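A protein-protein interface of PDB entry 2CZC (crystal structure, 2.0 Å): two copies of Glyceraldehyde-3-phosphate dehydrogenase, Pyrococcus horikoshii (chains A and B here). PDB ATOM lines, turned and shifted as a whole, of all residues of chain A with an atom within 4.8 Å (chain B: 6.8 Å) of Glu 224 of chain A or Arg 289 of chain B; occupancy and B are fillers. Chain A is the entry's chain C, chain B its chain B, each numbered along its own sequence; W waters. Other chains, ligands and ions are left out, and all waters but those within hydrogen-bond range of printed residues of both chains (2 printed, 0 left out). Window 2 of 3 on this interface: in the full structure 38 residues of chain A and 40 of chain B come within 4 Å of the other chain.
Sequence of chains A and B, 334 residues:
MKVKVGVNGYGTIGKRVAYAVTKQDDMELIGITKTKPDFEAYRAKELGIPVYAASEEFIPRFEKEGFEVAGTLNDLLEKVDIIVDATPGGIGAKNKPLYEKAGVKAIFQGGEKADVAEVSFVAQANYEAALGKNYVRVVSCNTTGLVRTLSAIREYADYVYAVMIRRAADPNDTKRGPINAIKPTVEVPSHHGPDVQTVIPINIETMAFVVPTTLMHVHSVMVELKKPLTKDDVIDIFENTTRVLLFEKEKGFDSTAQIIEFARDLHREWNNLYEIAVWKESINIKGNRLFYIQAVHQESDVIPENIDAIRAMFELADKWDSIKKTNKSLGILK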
ATOM      1  N   TYR A 156      31.571  22.152 -17.928  1.00  0.00           N
ATOM      2  CA  TYR A 156      31.555  20.720 -18.247  1.00  0.00           C
ATOM      3  C   TYR A 156      30.573  19.971 -17.366  1.00  0.00           C
ATOM      4  O   TYR A 156      30.272  18.801 -17.607  1.00  0.00           O
ATOM      5  CB  TYR A 156      32.933  20.090 -18.058  1.00  0.00           C
ATOM      6  CG  TYR A 156      34.086  20.870 -18.646  1.00  0.00           C
ATOM      7  CD1 TYR A 156      34.600  21.989 -17.985  1.00  0.00           C
ATOM      8  CD2 TYR A 156      34.693  20.468 -19.844  1.00  0.00           C
ATOM      9  CE1 TYR A 156      35.693  22.685 -18.495  1.00  0.00           C
ATOM     10  CE2 TYR A 156      35.781  21.161 -20.367  1.00  0.00           C
ATOM     11  CZ  TYR A 156      36.276  22.268 -19.682  1.00  0.00           C
ATOM     12  OH  TYR A 156      37.353  22.966 -20.179  1.00  0.00           O
ATOM     13  N   ALA A 157      30.077  20.654 -16.344  1.00  0.00           N
ATOM     14  CA  ALA A 157      29.159  20.058 -15.390  1.00  0.00           C
ATOM     15  C   ALA A 157      27.720  20.022 -15.865  1.00  0.00           C
ATOM     16  O   ALA A 157      27.120  21.056 -16.160  1.00  0.00           O
ATOM     17  CB  ALA A 157      29.237  20.813 -14.067  1.00  0.00           C
ATOM     18  N   ASP A 158      27.170  18.820 -15.938  1.00  0.00           N
ATOM     19  CA  ASP A 158      25.780  18.639 -16.326  1.00  0.00           C
ATOM     20  C   ASP A 158      24.966  18.453 -15.049  1.00  0.00           C
ATOM     21  O   ASP A 158      23.809  18.884 -14.945  1.00  0.00           O
ATOM     22  CB  ASP A 158      25.625  17.395 -17.177  1.00  0.00           C
ATOM     23  CG  ASP A 158      24.379  17.435 -18.016  1.00  0.00           C
ATOM     24  OD1 ASP A 158      24.009  16.383 -18.577  1.00  0.00           O
ATOM     25  OD2 ASP A 158      23.777  18.530 -18.117  1.00  0.00           O
ATOM     26  N   TYR A 159      25.586  17.784 -14.083  1.00  0.00           N
ATOM     27  CA  TYR A 159      24.966  17.521 -12.794  1.00  0.00           C
ATOM     28  C   TYR A 159      26.058  17.259 -11.763  1.00  0.00           C
ATOM     29  O   TYR A 159      27.080  16.636 -12.066  1.00  0.00           O
ATOM     30  CB  TYR A 159      24.054  16.292 -12.877  1.00  0.00           C
ATOM     31  CG  TYR A 159      23.437  15.908 -11.544  1.00  0.00           C
ATOM     32  CD1 TYR A 159      22.420  16.677 -10.970  1.00  0.00           C
ATOM     33  CD2 TYR A 159      23.909  14.807 -10.832  1.00  0.00           C
ATOM     34  CE1 TYR A 159      21.883  16.355  -9.699  1.00  0.00           C
ATOM     35  CE2 TYR A 159      23.386  14.475  -9.569  1.00  0.00           C
ATOM     36  CZ  TYR A 159      22.376  15.251  -9.012  1.00  0.00           C
ATOM     37  OH  TYR A 159      21.858  14.907  -7.777  1.00  0.00           O
ATOM     38  N   GLU A 205      22.750  18.759  -6.202  1.00  0.00           N
ATOM     39  CA  GLU A 205      22.039  18.280  -5.038  1.00  0.00           C
ATOM     40  C   GLU A 205      23.144  17.852  -4.079  1.00  0.00           C
ATOM     41  O   GLU A 205      24.160  17.275  -4.488  1.00  0.00           O
ATOM     42  CB  GLU A 205      21.078  17.159  -5.416  1.00  0.00           C
ATOM     43  CG  GLU A 205      19.953  17.735  -6.283  1.00  0.00           C
ATOM     44  CD  GLU A 205      19.011  16.709  -6.807  1.00  0.00           C
ATOM     45  OE1 GLU A 205      19.489  15.672  -7.326  1.00  0.00           O
ATOM     46  OE2 GLU A 205      17.784  16.953  -6.713  1.00  0.00           O
ATOM     47  N   MET A 222      31.127  14.613  -6.941  1.00  0.00           N
ATOM     48  CA  MET A 222      30.965  13.793  -8.129  1.00  0.00           C
ATOM     49  C   MET A 222      30.306  14.703  -9.164  1.00  0.00           C
ATOM     50  O   MET A 222      29.338  15.415  -8.849  1.00  0.00           O
ATOM     51  CB  MET A 222      30.098  12.575  -7.826  1.00  0.00           C
ATOM     52  CG  MET A 222      29.986  11.593  -8.973  1.00  0.00           C
ATOM     53  SD  MET A 222      28.636  12.046 -10.080  1.00  0.00           S
ATOM     54  CE  MET A 222      27.254  11.144  -9.292  1.00  0.00           C
ATOM     55  N   VAL A 223      30.851  14.705 -10.383  1.00  0.00           N
ATOM     56  CA  VAL A 223      30.328  15.556 -11.433  1.00  0.00           C
ATOM     57  C   VAL A 223      30.061  14.812 -12.743  1.00  0.00           C
ATOM     58  O   VAL A 223      30.954  14.182 -13.327  1.00  0.00           O
ATOM     59  CB  VAL A 223      31.284  16.728 -11.699  1.00  0.00           C
ATOM     60  CG1 VAL A 223      30.730  17.613 -12.806  1.00  0.00           C
ATOM     61  CG2 VAL A 223      31.469  17.543 -10.412  1.00  0.00           C
ATOM     62  N   GLU A 224      28.809  14.874 -13.172  1.00  0.00           N
ATOM     63  CA  GLU A 224      28.369  14.254 -14.410  1.00  0.00           C
ATOM     64  C   GLU A 224      28.742  15.235 -15.527  1.00  0.00           C
ATOM     65  O   GLU A 224      28.287  16.367 -15.542  1.00  0.00           O
ATOM     66  CB  GLU A 224      26.874  14.053 -14.331  1.00  0.00           C
ATOM     67  CG  GLU A 224      26.264  13.269 -15.447  1.00  0.00           C
ATOM     68  CD  GLU A 224      24.796  13.038 -15.172  1.00  0.00           C
ATOM     69  OE1 GLU A 224      24.496  12.393 -14.132  1.00  0.00           O
ATOM     70  OE2 GLU A 224      23.960  13.518 -15.974  1.00  0.00           O
ATOM     71  N   LEU A 225      29.570  14.791 -16.458  1.00  0.00           N
ATOM     72  CA  LEU A 225      30.058  15.657 -17.522  1.00  0.00           C
ATOM     73  C   LEU A 225      29.180  15.770 -18.765  1.00  0.00           C
ATOM     74  O   LEU A 225      28.504  14.822 -19.145  1.00  0.00           O
ATOM     75  CB  LEU A 225      31.458  15.191 -17.917  1.00  0.00           C
ATOM     76  CG  LEU A 225      32.452  15.124 -16.742  1.00  0.00           C
ATOM     77  CD1 LEU A 225      33.755  14.463 -17.171  1.00  0.00           C
ATOM     78  CD2 LEU A 225      32.715  16.527 -16.233  1.00  0.00           C
ATOM     79  N   LYS A 226      29.214  16.943 -19.389  1.00  0.00           N
ATOM     80  CA  LYS A 226      28.454  17.202 -20.608  1.00  0.00           C
ATOM     81  C   LYS A 226      29.396  17.601 -21.744  1.00  0.00           C
ATOM     82  O   LYS A 226      28.954  17.926 -22.846  1.00  0.00           O
ATOM     83  CB  LYS A 226      27.429  18.315 -20.380  1.00  0.00           C
ATOM     84  CG  LYS A 226      28.022  19.649 -19.972  1.00  0.00           C
ATOM     85  CD  LYS A 226      26.897  20.647 -19.666  1.00  0.00           C
ATOM     86  CE  LYS A 226      27.426  21.917 -19.006  1.00  0.00           C
ATOM     87  NZ  LYS A 226      26.335  22.787 -18.482  1.00  0.00           N
ATOM     88  N   ASN A 288      31.715   8.836 -17.719  1.00  0.00           N
ATOM     89  CA  ASN A 288      31.230  10.175 -17.865  1.00  0.00           C
ATOM     90  C   ASN A 288      31.120  10.949 -16.570  1.00  0.00           C
ATOM     91  O   ASN A 288      30.315  11.872 -16.471  1.00  0.00           O
ATOM     92  CB  ASN A 288      29.884  10.110 -18.519  1.00  0.00           C
ATOM     93  CG  ASN A 288      29.834  10.933 -19.718  1.00  0.00           C
ATOM     94  OD1 ASN A 288      30.307  10.529 -20.779  1.00  0.00           O
ATOM     95  ND2 ASN A 288      29.228  12.103 -19.593  1.00  0.00           N
ATOM     96  N   ARG A 289      31.941  10.596 -15.592  1.00  0.00           N
ATOM     97  CA  ARG A 289      31.856  11.253 -14.305  1.00  0.00           C
ATOM     98  C   ARG A 289      33.205  11.589 -13.708  1.00  0.00           C
ATOM     99  O   ARG A 289      34.127  10.776 -13.706  1.00  0.00           O
ATOM    100  CB  ARG A 289      31.058  10.368 -13.340  1.00  0.00           C
ATOM    101  CG  ARG A 289      30.043   9.472 -14.041  1.00  0.00           C
ATOM    102  CD  ARG A 289      29.130   8.768 -13.054  1.00  0.00           C
ATOM    103  NE  ARG A 289      27.961   9.586 -12.805  1.00  0.00           N
ATOM    104  CZ  ARG A 289      26.726   9.280 -13.189  1.00  0.00           C
ATOM    105  NH1 ARG A 289      26.487   8.149 -13.846  1.00  0.00           N
ATOM    106  NH2 ARG A 289      25.730  10.134 -12.930  1.00  0.00           N
ATOM    107  N   MET B 222      23.226   7.503  -3.516  1.00  0.00           N
ATOM    108  CA  MET B 222      22.488   8.111  -4.624  1.00  0.00           C
ATOM    109  C   MET B 222      22.295   7.002  -5.663  1.00  0.00           C
ATOM    110  O   MET B 222      23.246   6.278  -6.002  1.00  0.00           O
ATOM    111  CB  MET B 222      23.271   9.265  -5.256  1.00  0.00           C
ATOM    112  CG  MET B 222      22.524   9.930  -6.416  1.00  0.00           C
ATOM    113  SD  MET B 222      23.630  10.678  -7.657  1.00  0.00           S
ATOM    114  CE  MET B 222      23.582   9.452  -8.916  1.00  0.00           C
ATOM    115  N   VAL B 223      21.073   6.867  -6.163  1.00  0.00           N
ATOM    116  CA  VAL B 223      20.769   5.844  -7.156  1.00  0.00           C
ATOM    117  C   VAL B 223      20.048   6.441  -8.359  1.00  0.00           C
ATOM    118  O   VAL B 223      18.990   7.063  -8.202  1.00  0.00           O
ATOM    119  CB  VAL B 223      19.856   4.740  -6.569  1.00  0.00           C
ATOM    120  CG1 VAL B 223      19.717   3.601  -7.572  1.00  0.00           C
ATOM    121  CG2 VAL B 223      20.417   4.229  -5.255  1.00  0.00           C
ATOM    122  N   GLU B 224      20.612   6.260  -9.552  1.00  0.00           N
ATOM    123  CA  GLU B 224      19.970   6.765 -10.769  1.00  0.00           C
ATOM    124  C   GLU B 224      18.986   5.683 -11.170  1.00  0.00           C
ATOM    125  O   GLU B 224      19.365   4.532 -11.373  1.00  0.00           O
ATOM    126  CB  GLU B 224      20.994   6.994 -11.882  1.00  0.00           C
ATOM    127  CG  GLU B 224      22.198   7.773 -11.405  1.00  0.00           C
ATOM    128  CD  GLU B 224      22.709   8.766 -12.430  1.00  0.00           C
ATOM    129  OE1 GLU B 224      22.922   8.367 -13.597  1.00  0.00           O
ATOM    130  OE2 GLU B 224      22.905   9.944 -12.052  1.00  0.00           O
ATOM    131  N   LEU B 225      17.723   6.066 -11.275  1.00  0.00           N
ATOM    132  CA  LEU B 225      16.657   5.129 -11.584  1.00  0.00           C
ATOM    133  C   LEU B 225      16.493   4.847 -13.063  1.00  0.00           C
ATOM    134  O   LEU B 225      16.641   5.739 -13.891  1.00  0.00           O
ATOM    135  CB  LEU B 225      15.335   5.666 -11.019  1.00  0.00           C
ATOM    136  CG  LEU B 225      15.323   6.092  -9.549  1.00  0.00           C
ATOM    137  CD1 LEU B 225      14.069   6.905  -9.267  1.00  0.00           C
ATOM    138  CD2 LEU B 225      15.377   4.860  -8.647  1.00  0.00           C
ATOM    139  N   LEU B 229       9.995   5.111  -9.561  1.00  0.00           N
ATOM    140  CA  LEU B 229       9.909   4.615  -8.195  1.00  0.00           C
ATOM    141  C   LEU B 229       9.579   5.802  -7.301  1.00  0.00           C
ATOM    142  O   LEU B 229      10.152   6.875  -7.442  1.00  0.00           O
ATOM    143  CB  LEU B 229      11.254   4.007  -7.802  1.00  0.00           C
ATOM    144  CG  LEU B 229      11.406   3.297  -6.466  1.00  0.00           C
ATOM    145  CD1 LEU B 229      10.613   2.024  -6.487  1.00  0.00           C
ATOM    146  CD2 LEU B 229      12.874   2.983  -6.223  1.00  0.00           C
ATOM    147  N   ASN B 284      14.510  10.111  -0.254  1.00  0.00           N
ATOM    148  CA  ASN B 284      13.927  11.127  -1.122  1.00  0.00           C
ATOM    149  C   ASN B 284      14.135  10.840  -2.602  1.00  0.00           C
ATOM    150  O   ASN B 284      15.141  10.255  -3.000  1.00  0.00           O
ATOM    151  CB  ASN B 284      14.522  12.502  -0.809  1.00  0.00           C
ATOM    152  CG  ASN B 284      14.172  12.994   0.584  1.00  0.00           C
ATOM    153  OD1 ASN B 284      13.033  13.389   0.852  1.00  0.00           O
ATOM    154  ND2 ASN B 284      15.155  12.982   1.480  1.00  0.00           N
ATOM    155  N   ILE B 285      13.179  11.280  -3.409  1.00  0.00           N
ATOM    156  CA  ILE B 285      13.236  11.102  -4.850  1.00  0.00           C
ATOM    157  C   ILE B 285      13.257  12.471  -5.506  1.00  0.00           C
ATOM    158  O   ILE B 285      12.351  13.271  -5.298  1.00  0.00           O
ATOM    159  CB  ILE B 285      12.013  10.346  -5.369  1.00  0.00           C
ATOM    160  CG1 ILE B 285      12.001   8.926  -4.804  1.00  0.00           C
ATOM    161  CG2 ILE B 285      12.045  10.292  -6.891  1.00  0.00           C
ATOM    162  CD1 ILE B 285      13.065   8.043  -5.377  1.00  0.00           C
ATOM    163  N   LYS B 286      14.296  12.735  -6.291  1.00  0.00           N
ATOM    164  CA  LYS B 286      14.446  14.006  -6.979  1.00  0.00           C
ATOM    165  C   LYS B 286      14.752  13.697  -8.425  1.00  0.00           C
ATOM    166  O   LYS B 286      15.838  13.203  -8.744  1.00  0.00           O
ATOM    167  CB  LYS B 286      15.592  14.822  -6.378  1.00  0.00           C
ATOM    168  CG  LYS B 286      15.315  15.381  -4.991  1.00  0.00           C
ATOM    169  CD  LYS B 286      13.991  16.150  -4.964  1.00  0.00           C
ATOM    170  CE  LYS B 286      13.959  17.181  -3.849  1.00  0.00           C
ATOM    171  NZ  LYS B 286      14.879  18.322  -4.151  1.00  0.00           N
ATOM    172  N   GLY B 287      13.795  13.994  -9.301  1.00  0.00           N
ATOM    173  CA  GLY B 287      13.983  13.713 -10.709  1.00  0.00           C
ATOM    174  C   GLY B 287      14.058  12.212 -10.921  1.00  0.00           C
ATOM    175  O   GLY B 287      13.184  11.464 -10.483  1.00  0.00           O
ATOM    176  N   ASN B 288      15.109  11.757 -11.586  1.00  0.00           N
ATOM    177  CA  ASN B 288      15.261  10.326 -11.835  1.00  0.00           C
ATOM    178  C   ASN B 288      16.238   9.729 -10.818  1.00  0.00           C
ATOM    179  O   ASN B 288      16.823   8.674 -11.059  1.00  0.00           O
ATOM    180  CB  ASN B 288      15.789  10.097 -13.256  1.00  0.00           C
ATOM    181  CG  ASN B 288      17.239  10.559 -13.427  1.00  0.00           C
ATOM    182  OD1 ASN B 288      17.599  11.686 -13.060  1.00  0.00           O
ATOM    183  ND2 ASN B 288      18.075   9.689 -13.995  1.00  0.00           N
ATOM    184  N   ARG B 289      16.409  10.415  -9.689  1.00  0.00           N
ATOM    185  CA  ARG B 289      17.338   9.962  -8.656  1.00  0.00           C
ATOM    186  C   ARG B 289      16.707   9.666  -7.295  1.00  0.00           C
ATOM    187  O   ARG B 289      15.782  10.360  -6.849  1.00  0.00           O
ATOM    188  CB  ARG B 289      18.460  10.991  -8.486  1.00  0.00           C
ATOM    189  CG  ARG B 289      19.312  11.178  -9.725  1.00  0.00           C
ATOM    190  CD  ARG B 289      20.434  12.171  -9.477  1.00  0.00           C
ATOM    191  NE  ARG B 289      21.287  12.321 -10.654  1.00  0.00           N
ATOM    192  CZ  ARG B 289      20.969  13.046 -11.723  1.00  0.00           C
ATOM    193  NH1 ARG B 289      21.805  13.117 -12.753  1.00  0.00           N
ATOM    194  NH2 ARG B 289      19.829  13.723 -11.753  1.00  0.00           N
ATOM    195  N   LEU B 290      17.214   8.621  -6.646  1.00  0.00           N
ATOM    196  CA  LEU B 290      16.765   8.205  -5.318  1.00  0.00           C
ATOM    197  C   LEU B 290      17.922   8.485  -4.364  1.00  0.00           C
ATOM    198  O   LEU B 290      19.069   8.191  -4.711  1.00  0.00           O
ATOM    199  CB  LEU B 290      16.498   6.701  -5.292  1.00  0.00           C
ATOM    200  CG  LEU B 290      15.683   6.047  -4.177  1.00  0.00           C
ATOM    201  CD1 LEU B 290      16.137   4.606  -4.060  1.00  0.00           C
ATOM    202  CD2 LEU B 290      15.841   6.734  -2.845  1.00  0.00           C
ATOM    203  N   PHE B 291      17.626   9.067  -3.195  1.00  0.00           N
ATOM    204  CA  PHE B 291      18.642   9.339  -2.178  1.00  0.00           C
ATOM    205  C   PHE B 291      18.175   8.752  -0.853  1.00  0.00           C
ATOM    206  O   PHE B 291      16.973   8.741  -0.554  1.00  0.00           O
ATOM    207  CB  PHE B 291      18.861  10.848  -1.944  1.00  0.00           C
ATOM    208  CG  PHE B 291      19.278  11.611  -3.174  1.00  0.00           C
ATOM    209  CD1 PHE B 291      18.324  12.131  -4.045  1.00  0.00           C
ATOM    210  CD2 PHE B 291      20.627  11.807  -3.460  1.00  0.00           C
ATOM    211  CE1 PHE B 291      18.715  12.840  -5.187  1.00  0.00           C
ATOM    212  CE2 PHE B 291      21.030  12.517  -4.605  1.00  0.00           C
ATOM    213  CZ  PHE B 291      20.071  13.031  -5.465  1.00  0.00           C
HETATM  214  O   HOH W   1      18.260  14.588  -9.585  1.00  0.00           O
HETATM  215  O   HOH W   2      21.283  15.058 -14.942  1.00  0.00           O
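Glu 224 of chain A touches its own counterpart, Glu 224 of chain B. Glu 224 of chain A touches Arg 289 of chain B, and with the chains exchanged Arg 289 of chain A touches Glu 224 of chain B. 6 positions are printed for both chains.
Glu 224 of chain A touches just these residues of chain B: Glu 224 and Arg 289. Printed residues of chain A within 4 Å of Glu 224 of chain B: Glu 224 and Arg 289. Of the printed residues of chain B, Tyr 159 of chain A touches Arg 289 and Phe 291. Of the printed residues of chain A, Lys 286 of chain B touches Glu 205. Of the printed residues of chain B, Arg 289 of chain A touches Glu 224. Of the printed residues of chain B, Glu 205 of chain A touches Lys 286 and Phe 291. Val 223 of chain B touches none of the printed residues of chain A. Leu 229 of chain B touches none of the printed residues of chain A.
Hydrophobic or aromatic side chains of chain A that line the printed part of chain B: Tyr 159. Among the printed residues, 7 pairs touch across the chains.
Among the printed residues, pairs that only touch across the chains: Glu 205 of chain A with Lys 286 of chain B, Tyr 159 of chain A with Arg 289 of chain B, Glu 205 of chain A with Phe 291 of chain B, Tyr 159 of chain A with Phe 291 of chain B and Glu 224 of chain A with Glu 224 of chain B.
The side-chain carboxylate of Glu 224 of chain B is in salt-bridge range of the guanidinium group of Arg 289 of chain A (3.0 Å). The side-chain carboxylate (OE1) of Glu 224 of chain A lies within salt-bridge range of the guanidinium group (NH1) of Arg 289 of chain B, 3.1 Å away.
Water W1 lies within hydrogen-bond range of OE1 of Glu 205 of chain A (2.8 Å), NH2 of Arg 289 of chain B (2.8 Å) and O of Lys 286 of chain B (2.9 Å). Water W2 bridges the guanidinium group of Arg 289 of chain B (3.0 Å) and the side-chain carboxylate of Glu 224 of chain A (3.3 Å).
The guanidinium group (NE) of Arg 289 of chain B lies within salt-bridge range of the side-chain carboxylate (OE2) of Glu 224 of chain B. O of Asn 284 of chain B sits at hydrogen-bond distance from N of Phe 291 of chain B, at 2.8 Å. The guanidinium group (NH2) of Arg 289 of chain B sits at hydrogen-bond distance from the side-chain amide oxygen (OD1) of Asn 288 of chain B. The backbone carbonyl oxygen of Glu 224 of chain A lies within hydrogen-bond range of the backbone NH of Asp 158 of chain A. NE of Arg 289 of chain A sits at hydrogen-bond distance from SD of Met 222 of chain A (3.7 Å). The side-chain carboxylate of Glu 224 of chain A is in salt-bridge range of the guanidinium group of Arg 289 of chain A (2.8 Å).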
